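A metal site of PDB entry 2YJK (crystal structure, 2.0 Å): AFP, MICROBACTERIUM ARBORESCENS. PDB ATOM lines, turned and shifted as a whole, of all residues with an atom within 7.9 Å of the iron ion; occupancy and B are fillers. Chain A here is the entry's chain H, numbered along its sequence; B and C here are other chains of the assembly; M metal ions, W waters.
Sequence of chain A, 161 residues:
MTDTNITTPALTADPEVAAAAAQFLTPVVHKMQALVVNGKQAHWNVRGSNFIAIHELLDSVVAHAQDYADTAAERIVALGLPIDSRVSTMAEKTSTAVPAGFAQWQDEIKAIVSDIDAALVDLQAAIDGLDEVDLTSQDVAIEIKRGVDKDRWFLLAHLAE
The side-chain amino group (NZ) of Lys 150 of chain C lies within salt-bridge range of the side-chain carboxylate (OE1) of Glu 74, at 3.8 Å. NE2 of His 43 of chain B lies close to OD1 of Asp 59 of chain B (3.4 Å). A ring nitrogen (ND1) of His 43 of chain B lies within hydrogen-bond range of the backbone carbonyl oxygen of His 55 of chain B (2.7 Å). The side-chain carboxylate (OD1) of Asp 70 lies close to the indole nitrogen (NE1) of Trp 44 of chain B (2.9 Å). The side-chain amino group (NZ) of Lys 40 of chain B lies close to the side-chain carboxylate (OD1) of Asp 70 (3.1 Å).
Three residues have an atom within 4 Å of the iron ion: Asp 70, Glu 74 and His 43 of chain B.
The iron ion is bound by OE2 of Glu 74 (2.1 Å), NE2 of His 43 of chain B (2.3 Å), OD1 of Asp 70 (2.3 Å), water W1 (2.4 Å) and OD2 of Asp 70 (2.5 Å).
Water W1 lies within hydrogen-bond range of OE1 of Glu 74 (3.2 Å) and NE2 of His 55 of chain B (3.2 Å).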
ATOM      1  N   GLN A  66       3.469  -8.873  34.999  1.00  0.00           N
ATOM      2  CA  GLN A  66       4.483  -8.348  34.112  1.00  0.00           C
ATOM      3  C   GLN A  66       5.746  -9.290  34.115  1.00  0.00           C
ATOM      4  O   GLN A  66       6.330  -9.540  33.052  1.00  0.00           O
ATOM      5  CB  GLN A  66       4.892  -6.932  34.498  1.00  0.00           C
ATOM      6  CG  GLN A  66       5.854  -6.305  33.455  1.00  0.00           C
ATOM      7  CD  GLN A  66       5.272  -6.285  31.961  1.00  0.00           C
ATOM      8  OE1 GLN A  66       5.589  -7.175  31.095  1.00  0.00           O
ATOM      9  NE2 GLN A  66       4.554  -5.233  31.649  1.00  0.00           N
ATOM     10  N   ASP A  67       6.169  -9.764  35.296  1.00  0.00           N
ATOM     11  CA  ASP A  67       7.297 -10.719  35.349  1.00  0.00           C
ATOM     12  C   ASP A  67       6.988 -12.066  34.654  1.00  0.00           C
ATOM     13  O   ASP A  67       7.845 -12.600  33.996  1.00  0.00           O
ATOM     14  CB  ASP A  67       7.708 -10.986  36.797  1.00  0.00           C
ATOM     15  CG  ASP A  67       8.452  -9.814  37.394  1.00  0.00           C
ATOM     16  OD1 ASP A  67       9.160  -9.085  36.653  1.00  0.00           O
ATOM     17  OD2 ASP A  67       8.305  -9.606  38.627  1.00  0.00           O
ATOM     18  N   ALA A  69       4.780 -12.518  32.093  1.00  0.00           N
ATOM     19  CA  ALA A  69       4.766 -12.258  30.673  1.00  0.00           C
ATOM     20  C   ALA A  69       6.191 -12.319  30.217  1.00  0.00           C
ATOM     21  O   ALA A  69       6.474 -12.975  29.197  1.00  0.00           O
ATOM     22  CB  ALA A  69       4.138 -10.882  30.328  1.00  0.00           C
ATOM     23  N   ASP A  70       7.102 -11.627  30.938  1.00  0.00           N
ATOM     24  CA  ASP A  70       8.524 -11.526  30.457  1.00  0.00           C
ATOM     25  C   ASP A  70       9.160 -12.919  30.422  1.00  0.00           C
ATOM     26  O   ASP A  70       9.903 -13.251  29.488  1.00  0.00           O
ATOM     27  CB  ASP A  70       9.319 -10.568  31.390  1.00  0.00           C
ATOM     28  CG  ASP A  70      10.660 -10.093  30.806  1.00  0.00           C
ATOM     29  OD1 ASP A  70      10.664  -9.147  29.916  1.00  0.00           O
ATOM     30  OD2 ASP A  70      11.754 -10.625  31.277  1.00  0.00           O
ATOM     31  N   THR A  71       8.944 -13.725  31.470  1.00  0.00           N
ATOM     32  CA  THR A  71       9.530 -15.056  31.543  1.00  0.00           C
ATOM     33  C   THR A  71       9.024 -15.985  30.417  1.00  0.00           C
ATOM     34  O   THR A  71       9.836 -16.682  29.775  1.00  0.00           O
ATOM     35  CB  THR A  71       9.231 -15.690  32.945  1.00  0.00           C
ATOM     36  OG1 THR A  71       9.845 -14.821  33.889  1.00  0.00           O
ATOM     37  CG2 THR A  71       9.933 -16.991  33.095  1.00  0.00           C
ATOM     38  N   ALA A  73       7.615 -15.008  27.550  1.00  0.00           N
ATOM     39  CA  ALA A  73       8.071 -14.439  26.228  1.00  0.00           C
ATOM     40  C   ALA A  73       9.549 -14.743  25.915  1.00  0.00           C
ATOM     41  O   ALA A  73       9.934 -15.081  24.733  1.00  0.00           O
ATOM     42  CB  ALA A  73       7.817 -12.954  26.134  1.00  0.00           C
ATOM     43  N   GLU A  74      10.390 -14.670  26.948  1.00  0.00           N
ATOM     44  CA  GLU A  74      11.818 -14.879  26.734  1.00  0.00           C
ATOM     45  C   GLU A  74      12.163 -16.351  26.557  1.00  0.00           C
ATOM     46  O   GLU A  74      13.126 -16.666  25.942  1.00  0.00           O
ATOM     47  CB  GLU A  74      12.590 -14.245  27.881  1.00  0.00           C
ATOM     48  CG  GLU A  74      12.506 -12.716  27.637  1.00  0.00           C
ATOM     49  CD  GLU A  74      13.292 -11.863  28.621  1.00  0.00           C
ATOM     50  OE1 GLU A  74      13.952 -12.413  29.548  1.00  0.00           O
ATOM     51  OE2 GLU A  74      13.232 -10.629  28.442  1.00  0.00           O
ATOM     52  N   LYS B  40       8.018  -3.596  25.469  1.00  0.00           N
ATOM     53  CA  LYS B  40       8.338  -5.001  25.834  1.00  0.00           C
ATOM     54  C   LYS B  40       8.458  -5.842  24.544  1.00  0.00           C
ATOM     55  O   LYS B  40       9.322  -6.656  24.412  1.00  0.00           O
ATOM     56  CB  LYS B  40       7.268  -5.603  26.764  1.00  0.00           C
ATOM     57  CG  LYS B  40       7.344  -5.141  28.220  1.00  0.00           C
ATOM     58  CD  LYS B  40       8.695  -5.649  28.844  1.00  0.00           C
ATOM     59  CE  LYS B  40       8.761  -5.679  30.363  1.00  0.00           C
ATOM     60  NZ  LYS B  40      10.109  -6.209  30.844  1.00  0.00           N
ATOM     61  N   HIS B  43      11.872  -5.062  23.198  1.00  0.00           N
ATOM     62  CA  HIS B  43      12.829  -5.672  24.085  1.00  0.00           C
ATOM     63  C   HIS B  43      12.952  -7.212  23.862  1.00  0.00           C
ATOM     64  O   HIS B  43      14.078  -7.764  23.875  1.00  0.00           O
ATOM     65  CB  HIS B  43      12.259  -5.319  25.478  1.00  0.00           C
ATOM     66  CG  HIS B  43      12.867  -6.045  26.611  1.00  0.00           C
ATOM     67  ND1 HIS B  43      14.072  -5.663  27.168  1.00  0.00           N
ATOM     68  CD2 HIS B  43      12.371  -7.042  27.400  1.00  0.00           C
ATOM     69  CE1 HIS B  43      14.315  -6.429  28.232  1.00  0.00           C
ATOM     70  NE2 HIS B  43      13.322  -7.288  28.370  1.00  0.00           N
ATOM     71  N   TRP B  44      11.839  -7.900  23.680  1.00  0.00           N
ATOM     72  CA  TRP B  44      11.850  -9.352  23.414  1.00  0.00           C
ATOM     73  C   TRP B  44      12.442  -9.702  22.016  1.00  0.00           C
ATOM     74  O   TRP B  44      13.183 -10.671  21.893  1.00  0.00           O
ATOM     75  CB  TRP B  44      10.412  -9.926  23.483  1.00  0.00           C
ATOM     76  CG  TRP B  44       9.889  -9.846  24.953  1.00  0.00           C
ATOM     77  CD1 TRP B  44      10.660  -9.893  26.128  1.00  0.00           C
ATOM     78  CD2 TRP B  44       8.550  -9.649  25.370  1.00  0.00           C
ATOM     79  NE1 TRP B  44       9.831  -9.743  27.241  1.00  0.00           N
ATOM     80  CE2 TRP B  44       8.534  -9.635  26.798  1.00  0.00           C
ATOM     81  CE3 TRP B  44       7.325  -9.607  24.675  1.00  0.00           C
ATOM     82  CZ2 TRP B  44       7.344  -9.513  27.542  1.00  0.00           C
ATOM     83  CZ3 TRP B  44       6.140  -9.471  25.446  1.00  0.00           C
ATOM     84  CH2 TRP B  44       6.171  -9.440  26.832  1.00  0.00           C
ATOM     85  N   HIS B  55      18.513  -4.049  24.471  1.00  0.00           N
ATOM     86  CA  HIS B  55      17.572  -4.897  25.260  1.00  0.00           C
ATOM     87  C   HIS B  55      17.375  -4.203  26.639  1.00  0.00           C
ATOM     88  O   HIS B  55      16.207  -4.007  27.068  1.00  0.00           O
ATOM     89  CB  HIS B  55      18.171  -6.296  25.392  1.00  0.00           C
ATOM     90  CG  HIS B  55      17.379  -7.286  26.200  1.00  0.00           C
ATOM     91  ND1 HIS B  55      16.198  -7.838  25.746  1.00  0.00           N
ATOM     92  CD2 HIS B  55      17.612  -7.854  27.414  1.00  0.00           C
ATOM     93  CE1 HIS B  55      15.754  -8.729  26.640  1.00  0.00           C
ATOM     94  NE2 HIS B  55      16.584  -8.745  27.674  1.00  0.00           N
ATOM     95  N   ASP B  59      14.129  -1.927  28.325  1.00  0.00           N
ATOM     96  CA  ASP B  59      13.554  -2.219  29.639  1.00  0.00           C
ATOM     97  C   ASP B  59      13.403  -0.953  30.536  1.00  0.00           C
ATOM     98  O   ASP B  59      12.425  -0.753  31.210  1.00  0.00           O
ATOM     99  CB  ASP B  59      14.331  -3.334  30.380  1.00  0.00           C
ATOM    100  CG  ASP B  59      13.410  -4.565  30.737  1.00  0.00           C
ATOM    101  OD1 ASP B  59      12.226  -4.661  30.221  1.00  0.00           O
ATOM    102  OD2 ASP B  59      13.834  -5.468  31.497  1.00  0.00           O
ATOM    103  N   LYS C 150      18.875 -19.237  28.367  1.00  0.00           N
ATOM    104  CA  LYS C 150      18.694 -17.822  28.289  1.00  0.00           C
ATOM    105  C   LYS C 150      20.035 -17.084  28.025  1.00  0.00           C
ATOM    106  O   LYS C 150      20.098 -16.223  27.138  1.00  0.00           O
ATOM    107  CB  LYS C 150      18.018 -17.356  29.582  1.00  0.00           C
ATOM    108  CG  LYS C 150      17.976 -15.884  29.740  1.00  0.00           C
ATOM    109  CD  LYS C 150      17.085 -15.517  30.938  1.00  0.00           C
ATOM    110  CE  LYS C 150      16.704 -14.065  30.759  1.00  0.00           C
ATOM    111  NZ  LYS C 150      16.643 -13.346  32.025  1.00  0.00           N
ATOM    112  N   TRP C 153      20.913 -17.323  24.330  1.00  0.00           N
ATOM    113  CA  TRP C 153      20.191 -16.381  23.512  1.00  0.00           C
ATOM    114  C   TRP C 153      20.857 -14.947  23.622  1.00  0.00           C
ATOM    115  O   TRP C 153      21.073 -14.244  22.611  1.00  0.00           O
ATOM    116  CB  TRP C 153      18.723 -16.378  24.016  1.00  0.00           C
ATOM    117  CG  TRP C 153      17.947 -15.108  23.596  1.00  0.00           C
ATOM    118  CD1 TRP C 153      17.891 -14.553  22.331  1.00  0.00           C
ATOM    119  CD2 TRP C 153      17.130 -14.271  24.442  1.00  0.00           C
ATOM    120  NE1 TRP C 153      17.099 -13.410  22.360  1.00  0.00           N
ATOM    121  CE2 TRP C 153      16.633 -13.212  23.635  1.00  0.00           C
ATOM    122  CE3 TRP C 153      16.796 -14.293  25.822  1.00  0.00           C
ATOM    123  CZ2 TRP C 153      15.785 -12.190  24.150  1.00  0.00           C
ATOM    124  CZ3 TRP C 153      15.967 -13.281  26.328  1.00  0.00           C
ATOM    125  CH2 TRP C 153      15.467 -12.239  25.480  1.00  0.00           C
ATOM    126  N   PHE C 154      21.184 -14.545  24.838  1.00  0.00           N
ATOM    127  CA  PHE C 154      21.762 -13.223  25.099  1.00  0.00           C
ATOM    128  C   PHE C 154      23.082 -13.113  24.340  1.00  0.00           C
ATOM    129  O   PHE C 154      23.383 -12.065  23.825  1.00  0.00           O
ATOM    130  CB  PHE C 154      22.060 -13.026  26.592  1.00  0.00           C
ATOM    131  CG  PHE C 154      20.891 -12.492  27.394  1.00  0.00           C
ATOM    132  CD1 PHE C 154      19.619 -12.338  26.838  1.00  0.00           C
ATOM    133  CD2 PHE C 154      21.068 -12.164  28.741  1.00  0.00           C
ATOM    134  CE1 PHE C 154      18.542 -11.799  27.580  1.00  0.00           C
ATOM    135  CE2 PHE C 154      19.977 -11.636  29.528  1.00  0.00           C
ATOM    136  CZ  PHE C 154      18.717 -11.452  28.913  1.00  0.00           C
HETATM  137 FE    FE M   1      13.009  -9.055  29.858  1.00  0.00          FE
HETATM  138  O   HOH W   1      15.225  -9.633  30.482  1.00  0.00           O
